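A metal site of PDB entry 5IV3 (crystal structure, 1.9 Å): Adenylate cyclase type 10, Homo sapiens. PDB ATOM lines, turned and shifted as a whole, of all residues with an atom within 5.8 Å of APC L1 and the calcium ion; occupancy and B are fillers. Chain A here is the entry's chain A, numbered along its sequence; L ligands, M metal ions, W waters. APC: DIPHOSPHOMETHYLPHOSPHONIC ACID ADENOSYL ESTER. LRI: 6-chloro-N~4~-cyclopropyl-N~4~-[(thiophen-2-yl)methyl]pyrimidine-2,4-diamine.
The calcium ion is bound by OD1 of Asp 47 (2.3 Å). The calcium ion is bound by OD1 of Asp 99, at 2.3 Å. The calcium ion is bound by water W2. O of Ile 48 binds the calcium ion (2.5 Å). The calcium ion is bound by O1B of APC L1, 2.5 Å away. O2G of APC L1 is bound to the calcium ion, at 2.6 Å. The calcium ion has six donor atoms within binding distance.
The side-chain amide nitrogen (ND2) of Asn 412 lies within hydrogen-bond range of an oxygen (O1G) of APC L1 (3.0 Å). The backbone NH (N) of Phe 51 sits at hydrogen-bond distance from an oxygen (O3G) of APC L1, 3.2 Å away. OD1 of Asn 180 is in hydrogen-bond range of O3' of APC L1 (2.8 Å). An oxygen (O3G) of APC L1 lies within hydrogen-bond range of the backbone NH (N) of Gly 50 (2.8 Å). The guanidinium group of Arg 176 sits at hydrogen-bond distance from an oxygen (O2') of APC L1 (2.8 Å). NH2 of Arg 416 lies within salt-bridge range of O1A of APC L1, at 2.7 Å. The side-chain hydroxyl of Ser 49 lies within hydrogen-bond range of an oxygen (O2B) of APC L1. An oxygen (O3G) of APC L1 is in hydrogen-bond range of the backbone NH of Thr 52. The side-chain amide oxygen (OE1) of Gln 179 is in hydrogen-bond range of an oxygen (O2') of APC L1, at 2.8 Å.
Within 4 Å of the calcium ion: Asp 47, Ile 48 and Asp 99.
Residues that only touch APC L1: Phe 45 (3.8 Å), Ala 97 (3.4 Å) and Phe 338 (3.4 Å). Along chain A the residues within 4 Å of APC L1 span positions 45 to 416.
The backbone NH of Phe 51 sits close to the side-chain carboxylate of Asp 99, 3.5 Å away. The guanidinium group (NE) of Arg 416 sits at hydrogen-bond distance from the backbone carbonyl oxygen (O) of Lys 451 (2.9 Å). The side-chain carboxylate (OD2) of Asp 47 lies within hydrogen-bond range of the side-chain amide nitrogen (NE2) of Gln 179, 3.2 Å away. The backbone carbonyl oxygen (O) of Asp 47 is in hydrogen-bond range of the backbone NH (N) of Lys 144, at 2.9 Å.
Water W1 lies within hydrogen-bond range of N6 of APC L1 (2.4 Å) and O of Ala 97 (2.8 Å). Water W3 lies within hydrogen-bond range of O3G of APC L1 (2.6 Å), N of Ala 53 (2.9 Å) and N of Thr 52 (3.5 Å).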
ATOM      1  N   PHE A  45      -6.118   5.595  11.795  1.00  0.00           N
ATOM      2  CA  PHE A  45      -6.107   6.501  12.944  1.00  0.00           C
ATOM      3  C   PHE A  45      -4.719   6.970  13.148  1.00  0.00           C
ATOM      4  O   PHE A  45      -3.785   6.138  13.372  1.00  0.00           O
ATOM      5  CB  PHE A  45      -6.672   5.825  14.200  1.00  0.00           C
ATOM      6  CG  PHE A  45      -6.829   6.768  15.339  1.00  0.00           C
ATOM      7  CD1 PHE A  45      -7.484   8.010  15.173  1.00  0.00           C
ATOM      8  CD2 PHE A  45      -6.282   6.466  16.561  1.00  0.00           C
ATOM      9  CE1 PHE A  45      -7.572   8.890  16.218  1.00  0.00           C
ATOM     10  CE2 PHE A  45      -6.364   7.352  17.618  1.00  0.00           C
ATOM     11  CZ  PHE A  45      -7.021   8.543  17.463  1.00  0.00           C
ATOM     12  N   ASP A  47      -2.385   9.503  15.242  1.00  0.00           N
ATOM     13  CA  ASP A  47      -2.339  10.158  16.535  1.00  0.00           C
ATOM     14  C   ASP A  47      -0.970  10.737  16.715  1.00  0.00           C
ATOM     15  O   ASP A  47       0.030   9.982  16.815  1.00  0.00           O
ATOM     16  CB  ASP A  47      -2.614   9.185  17.666  1.00  0.00           C
ATOM     17  CG  ASP A  47      -2.630   9.868  19.025  1.00  0.00           C
ATOM     18  OD1 ASP A  47      -3.114  11.009  19.102  1.00  0.00           O
ATOM     19  OD2 ASP A  47      -2.196   9.272  20.032  1.00  0.00           O
ATOM     20  N   ILE A  48      -0.881  12.056  16.699  1.00  0.00           N
ATOM     21  CA  ILE A  48       0.369  12.752  17.045  1.00  0.00           C
ATOM     22  C   ILE A  48       0.523  12.702  18.568  1.00  0.00           C
ATOM     23  O   ILE A  48      -0.442  12.893  19.314  1.00  0.00           O
ATOM     24  CB  ILE A  48       0.392  14.231  16.663  1.00  0.00           C
ATOM     25  CG1 ILE A  48       0.038  14.464  15.179  1.00  0.00           C
ATOM     26  CG2 ILE A  48       1.721  14.874  17.069  1.00  0.00           C
ATOM     27  CD1 ILE A  48       0.892  13.766  14.174  1.00  0.00           C
ATOM     28  N   SER A  49       1.729  12.437  19.013  1.00  0.00           N
ATOM     29  CA  SER A  49       2.106  12.525  20.419  1.00  0.00           C
ATOM     30  C   SER A  49       3.029  13.776  20.492  1.00  0.00           C
ATOM     31  O   SER A  49       3.971  13.941  19.679  1.00  0.00           O
ATOM     32  CB  SER A  49       2.840  11.262  20.845  1.00  0.00           C
ATOM     33  OG  SER A  49       2.244  10.677  21.997  1.00  0.00           O
ATOM     34  N   GLY A  50       2.666  14.688  21.397  1.00  0.00           N
ATOM     35  CA  GLY A  50       3.498  15.751  21.873  1.00  0.00           C
ATOM     36  C   GLY A  50       2.824  17.091  21.820  1.00  0.00           C
ATOM     37  O   GLY A  50       3.358  18.043  22.390  1.00  0.00           O
ATOM     38  N   PHE A  51       1.688  17.267  21.138  1.00  0.00           N
ATOM     39  CA  PHE A  51       1.150  18.602  21.232  1.00  0.00           C
ATOM     40  C   PHE A  51       0.569  18.955  22.580  1.00  0.00           C
ATOM     41  O   PHE A  51       0.459  20.191  22.857  1.00  0.00           O
ATOM     42  CB  PHE A  51       0.215  18.988  20.129  1.00  0.00           C
ATOM     43  CG  PHE A  51       0.935  19.510  18.943  1.00  0.00           C
ATOM     44  CD1 PHE A  51       1.407  18.623  17.957  1.00  0.00           C
ATOM     45  CD2 PHE A  51       1.183  20.874  18.812  1.00  0.00           C
ATOM     46  CE1 PHE A  51       2.112  19.083  16.829  1.00  0.00           C
ATOM     47  CE2 PHE A  51       1.870  21.338  17.673  1.00  0.00           C
ATOM     48  CZ  PHE A  51       2.336  20.436  16.680  1.00  0.00           C
ATOM     49  N   THR A  52       0.164  17.977  23.428  1.00  0.00           N
ATOM     50  CA  THR A  52      -0.420  18.406  24.727  1.00  0.00           C
ATOM     51  C   THR A  52       0.666  19.037  25.600  1.00  0.00           C
ATOM     52  O   THR A  52       0.462  20.109  26.147  1.00  0.00           O
ATOM     53  CB  THR A  52      -1.261  17.368  25.499  1.00  0.00           C
ATOM     54  OG1 THR A  52      -1.844  18.010  26.641  1.00  0.00           O
ATOM     55  CG2 THR A  52      -0.438  16.262  26.025  1.00  0.00           C
ATOM     56  N   ALA A  53       1.865  18.450  25.666  1.00  0.00           N
ATOM     57  CA  ALA A  53       3.049  19.167  26.223  1.00  0.00           C
ATOM     58  C   ALA A  53       3.358  20.526  25.597  1.00  0.00           C
ATOM     59  O   ALA A  53       3.567  21.508  26.303  1.00  0.00           O
ATOM     60  CB  ALA A  53       4.299  18.307  26.116  1.00  0.00           C
ATOM     61  N   ALA A  97      -9.710  15.122  16.564  1.00  0.00           N
ATOM     62  CA  ALA A  97      -9.775  15.256  18.021  1.00  0.00           C
ATOM     63  C   ALA A  97      -8.414  15.651  18.485  1.00  0.00           C
ATOM     64  O   ALA A  97      -7.436  14.860  18.425  1.00  0.00           O
ATOM     65  CB  ALA A  97     -10.154  13.958  18.646  1.00  0.00           C
ATOM     66  N   ASP A  99      -4.968  16.535  18.496  1.00  0.00           N
ATOM     67  CA  ASP A  99      -3.883  16.308  17.523  1.00  0.00           C
ATOM     68  C   ASP A  99      -3.944  14.930  16.829  1.00  0.00           C
ATOM     69  O   ASP A  99      -2.886  14.399  16.377  1.00  0.00           O
ATOM     70  CB  ASP A  99      -2.518  16.538  18.219  1.00  0.00           C
ATOM     71  CG  ASP A  99      -2.287  15.624  19.387  1.00  0.00           C
ATOM     72  OD1 ASP A  99      -3.124  14.727  19.631  1.00  0.00           O
ATOM     73  OD2 ASP A  99      -1.349  15.881  20.138  1.00  0.00           O
ATOM     74  N   ALA A 100      -5.157  14.367  16.724  1.00  0.00           N
ATOM     75  CA  ALA A 100      -5.391  13.091  16.084  1.00  0.00           C
ATOM     76  C   ALA A 100      -6.484  13.234  15.079  1.00  0.00           C
ATOM     77  O   ALA A 100      -7.347  14.132  15.202  1.00  0.00           O
ATOM     78  CB  ALA A 100      -5.835  12.095  17.124  1.00  0.00           C
ATOM     79  N   LYS A 144       1.876   8.165  15.537  1.00  0.00           N
ATOM     80  CA  LYS A 144       1.551   6.753  15.608  1.00  0.00           C
ATOM     81  C   LYS A 144       0.343   6.479  14.706  1.00  0.00           C
ATOM     82  O   LYS A 144      -0.647   7.226  14.770  1.00  0.00           O
ATOM     83  CB  LYS A 144       1.219   6.349  17.036  1.00  0.00           C
ATOM     84  CG  LYS A 144       2.293   6.645  18.093  1.00  0.00           C
ATOM     85  CD  LYS A 144       1.805   6.239  19.498  1.00  0.00           C
ATOM     86  CE  LYS A 144       2.824   6.645  20.538  1.00  0.00           C
ATOM     87  NZ  LYS A 144       2.591   5.888  21.804  1.00  0.00           N
ATOM     88  N   ARG A 176      -8.182   1.703  16.760  1.00  0.00           N
ATOM     89  CA  ARG A 176      -7.695   2.371  17.962  1.00  0.00           C
ATOM     90  C   ARG A 176      -6.695   1.483  18.766  1.00  0.00           C
ATOM     91  O   ARG A 176      -5.632   1.975  19.204  1.00  0.00           O
ATOM     92  CB  ARG A 176      -8.823   2.816  18.840  1.00  0.00           C
ATOM     93  CG  ARG A 176      -8.310   4.015  19.643  1.00  0.00           C
ATOM     94  CD  ARG A 176      -8.655   3.994  21.079  1.00  0.00           C
ATOM     95  NE  ARG A 176      -8.488   2.695  21.727  1.00  0.00           N
ATOM     96  CZ  ARG A 176      -7.578   2.392  22.686  1.00  0.00           C
ATOM     97  NH1 ARG A 176      -7.621   1.188  23.243  1.00  0.00           N
ATOM     98  NH2 ARG A 176      -6.643   3.262  23.095  1.00  0.00           N
ATOM     99  N   GLN A 179      -3.248   1.483  16.718  1.00  0.00           N
ATOM    100  CA  GLN A 179      -2.500   2.707  16.879  1.00  0.00           C
ATOM    101  C   GLN A 179      -1.838   2.809  18.265  1.00  0.00           C
ATOM    102  O   GLN A 179      -0.744   3.344  18.424  1.00  0.00           O
ATOM    103  CB  GLN A 179      -3.446   3.942  16.679  1.00  0.00           C
ATOM    104  CG  GLN A 179      -2.821   5.258  17.134  1.00  0.00           C
ATOM    105  CD  GLN A 179      -3.122   5.561  18.585  1.00  0.00           C
ATOM    106  OE1 GLN A 179      -4.195   5.280  19.070  1.00  0.00           O
ATOM    107  NE2 GLN A 179      -2.220   6.138  19.244  1.00  0.00           N
ATOM    108  N   ASN A 180      -2.582   2.393  19.284  1.00  0.00           N
ATOM    109  CA  ASN A 180      -2.103   2.474  20.681  1.00  0.00           C
ATOM    110  C   ASN A 180      -0.848   1.587  20.993  1.00  0.00           C
ATOM    111  O   ASN A 180      -0.124   1.852  21.952  1.00  0.00           O
ATOM    112  CB  ASN A 180      -3.270   2.104  21.568  1.00  0.00           C
ATOM    113  CG  ASN A 180      -3.042   2.471  23.017  1.00  0.00           C
ATOM    114  OD1 ASN A 180      -2.614   3.561  23.320  1.00  0.00           O
ATOM    115  ND2 ASN A 180      -3.319   1.543  23.900  1.00  0.00           N
ATOM    116  N   PHE A 336     -17.020  10.580  20.613  1.00  0.00           N
ATOM    117  CA  PHE A 336     -16.104   9.465  20.268  1.00  0.00           C
ATOM    118  C   PHE A 336     -16.753   8.143  20.686  1.00  0.00           C
ATOM    119  O   PHE A 336     -17.530   8.118  21.641  1.00  0.00           O
ATOM    120  CB  PHE A 336     -14.859   9.476  21.129  1.00  0.00           C
ATOM    121  CG  PHE A 336     -14.210  10.758  21.218  1.00  0.00           C
ATOM    122  CD1 PHE A 336     -13.443  11.175  20.197  1.00  0.00           C
ATOM    123  CD2 PHE A 336     -14.389  11.579  22.320  1.00  0.00           C
ATOM    124  CE1 PHE A 336     -12.822  12.422  20.266  1.00  0.00           C
ATOM    125  CE2 PHE A 336     -13.746  12.786  22.417  1.00  0.00           C
ATOM    126  CZ  PHE A 336     -12.963  13.226  21.393  1.00  0.00           C
ATOM    127  N   PHE A 338     -15.300   3.856  21.148  1.00  0.00           N
ATOM    128  CA  PHE A 338     -14.415   2.662  20.921  1.00  0.00           C
ATOM    129  C   PHE A 338     -14.491   1.823  22.199  1.00  0.00           C
ATOM    130  O   PHE A 338     -14.947   2.347  23.216  1.00  0.00           O
ATOM    131  CB  PHE A 338     -12.991   3.050  20.571  1.00  0.00           C
ATOM    132  CG  PHE A 338     -12.400   4.045  21.515  1.00  0.00           C
ATOM    133  CD1 PHE A 338     -11.737   3.623  22.678  1.00  0.00           C
ATOM    134  CD2 PHE A 338     -12.471   5.412  21.236  1.00  0.00           C
ATOM    135  CE1 PHE A 338     -11.178   4.573  23.557  1.00  0.00           C
ATOM    136  CE2 PHE A 338     -11.898   6.352  22.115  1.00  0.00           C
ATOM    137  CZ  PHE A 338     -11.280   5.927  23.282  1.00  0.00           C
ATOM    138  N   ASN A 412      -6.944  15.664  28.690  1.00  0.00           N
ATOM    139  CA  ASN A 412      -6.406  14.350  28.931  1.00  0.00           C
ATOM    140  C   ASN A 412      -6.717  13.868  30.380  1.00  0.00           C
ATOM    141  O   ASN A 412      -7.077  12.694  30.576  1.00  0.00           O
ATOM    142  CB  ASN A 412      -4.878  14.301  28.722  1.00  0.00           C
ATOM    143  CG  ASN A 412      -4.488  14.489  27.253  1.00  0.00           C
ATOM    144  OD1 ASN A 412      -5.339  14.818  26.452  1.00  0.00           O
ATOM    145  ND2 ASN A 412      -3.222  14.259  26.924  1.00  0.00           N
ATOM    146  N   ARG A 416      -8.785  10.495  31.425  1.00  0.00           N
ATOM    147  CA  ARG A 416      -8.170   9.488  32.298  1.00  0.00           C
ATOM    148  C   ARG A 416      -8.980   9.204  33.572  1.00  0.00           C
ATOM    149  O   ARG A 416      -9.199   8.026  33.894  1.00  0.00           O
ATOM    150  CB  ARG A 416      -6.765   9.891  32.659  1.00  0.00           C
ATOM    151  CG  ARG A 416      -5.809   9.872  31.496  1.00  0.00           C
ATOM    152  CD  ARG A 416      -5.296   8.485  31.164  1.00  0.00           C
ATOM    153  NE  ARG A 416      -4.763   8.414  29.784  1.00  0.00           N
ATOM    154  CZ  ARG A 416      -5.350   7.813  28.732  1.00  0.00           C
ATOM    155  NH1 ARG A 416      -6.515   7.165  28.831  1.00  0.00           N
ATOM    156  NH2 ARG A 416      -4.738   7.840  27.558  1.00  0.00           N
ATOM    157  N   LYS A 451      -1.864   6.364  33.310  1.00  0.00           N
ATOM    158  CA  LYS A 451      -0.950   6.262  32.142  1.00  0.00           C
ATOM    159  C   LYS A 451      -0.997   7.535  31.286  1.00  0.00           C
ATOM    160  O   LYS A 451      -2.073   7.941  30.835  1.00  0.00           O
ATOM    161  CB  LYS A 451      -1.255   5.005  31.281  1.00  0.00           C
ATOM    162  N   GLY A 452       0.175   8.141  31.102  1.00  0.00           N
ATOM    163  CA  GLY A 452       0.296   9.446  30.464  1.00  0.00           C
ATOM    164  C   GLY A 452      -0.149  10.635  31.311  1.00  0.00           C
ATOM    165  O   GLY A 452      -0.602  11.637  30.763  1.00  0.00           O
HETATM  166  PG  APC L   1      -0.626  13.978  23.318  1.00  0.00           P
HETATM  167  O1G APC L   1      -1.655  14.101  24.364  1.00  0.00           O
HETATM  168  O2G APC L   1      -1.251  14.347  22.018  1.00  0.00           O
HETATM  169  O3G APC L   1       0.432  15.061  23.054  1.00  0.00           O
HETATM  170  PB  APC L   1      -1.045  11.126  23.161  1.00  0.00           P
HETATM  171  O1B APC L   1      -2.152  10.689  22.142  1.00  0.00           O
HETATM  172  O2B APC L   1       0.102  10.198  23.181  1.00  0.00           O
HETATM  173  O3B APC L   1      -0.163  12.486  22.987  1.00  0.00           O
HETATM  174  PA  APC L   1      -2.070   9.518  25.456  1.00  0.00           P
HETATM  175  O1A APC L   1      -2.824   9.591  26.877  1.00  0.00           O
HETATM  176  O2A APC L   1      -0.725   8.872  25.675  1.00  0.00           O
HETATM  177  C3A APC L   1      -1.942  11.181  24.727  1.00  0.00           C
HETATM  178  O5' APC L   1      -2.925   8.637  24.470  1.00  0.00           O
HETATM  179  C5' APC L   1      -2.842   7.262  24.912  1.00  0.00           C
HETATM  180  C4' APC L   1      -3.802   6.438  24.125  1.00  0.00           C
HETATM  181  O4' APC L   1      -5.178   6.800  24.332  1.00  0.00           O
HETATM  182  C3' APC L   1      -3.464   6.747  22.661  1.00  0.00           C
HETATM  183  O3' APC L   1      -2.256   6.083  22.278  1.00  0.00           O
HETATM  184  C2' APC L   1      -4.760   6.419  21.958  1.00  0.00           C
HETATM  185  O2' APC L   1      -4.936   5.027  21.707  1.00  0.00           O
HETATM  186  C1' APC L   1      -5.743   6.916  23.009  1.00  0.00           C
HETATM  187  N9  APC L   1      -6.095   8.317  22.574  1.00  0.00           N
HETATM  188  C8  APC L   1      -5.497   9.547  22.724  1.00  0.00           C
HETATM  189  N7  APC L   1      -6.251  10.493  22.112  1.00  0.00           N
HETATM  190  C5  APC L   1      -7.327   9.843  21.538  1.00  0.00           C
HETATM  191  C6  APC L   1      -8.557  10.122  20.742  1.00  0.00           C
HETATM  192  N6  APC L   1      -8.876  11.326  20.354  1.00  0.00           N
HETATM  193  N1  APC L   1      -9.416   9.157  20.400  1.00  0.00           N
HETATM  194  C2  APC L   1      -9.218   7.873  20.757  1.00  0.00           C
HETATM  195  N3  APC L   1      -8.146   7.517  21.469  1.00  0.00           N
HETATM  196  C4  APC L   1      -7.218   8.436  21.865  1.00  0.00           C
HETATM  197  CAL LRI L   2     -10.315   6.816  17.240  1.00  0.00           C
HETATM  198  CAM LRI L   2     -10.062   5.587  16.729  1.00  0.00           C
HETATM  199  CAN LRI L   2     -11.120   4.742  16.503  1.00  0.00           C
HETATM  200  SAO LRI L   2     -12.459   5.522  17.118  1.00  0.00           S
HETATM  201  CAK LRI L   2     -11.627   6.929  17.567  1.00  0.00           C
HETATM  202  CAJ LRI L   2     -12.382   8.121  18.176  1.00  0.00           C
HETATM  203  NAI LRI L   2     -12.913   9.002  17.148  1.00  0.00           N
HETATM  204  CAP LRI L   2     -11.885   9.821  16.467  1.00  0.00           C
HETATM  205  CAQ LRI L   2     -12.088  11.362  16.382  1.00  0.00           C
HETATM  206  CAR LRI L   2     -11.124  10.710  17.372  1.00  0.00           C
HETATM  207  C4  LRI L   2     -14.054   8.677  16.563  1.00  0.00           C
HETATM  208  N3  LRI L   2     -14.766   7.659  17.038  1.00  0.00           N
HETATM  209  C5  LRI L   2     -14.512   9.310  15.408  1.00  0.00           C
HETATM  210  C6  LRI L   2     -15.659   8.814  14.838  1.00  0.00           C
HETATM  211 CL6  LRI L   2     -16.297   9.471  13.400  1.00  0.00          CL
HETATM  212  N1  LRI L   2     -16.244   7.753  15.320  1.00  0.00           N
HETATM  213  C2  LRI L   2     -15.810   7.186  16.433  1.00  0.00           C
HETATM  214  NAA LRI L   2     -16.443   6.128  16.928  1.00  0.00           N
HETATM  215 CA    CA M   1      -2.548  12.664  20.590  1.00  0.00          CA
HETATM  216  O   HOH W   1      -7.158  13.029  20.535  1.00  0.00           O
HETATM  217  O   HOH W   2      -4.570  12.902  21.917  1.00  0.00           O
HETATM  218  O   HOH W   3       2.082  15.590  25.052  1.00  0.00           O
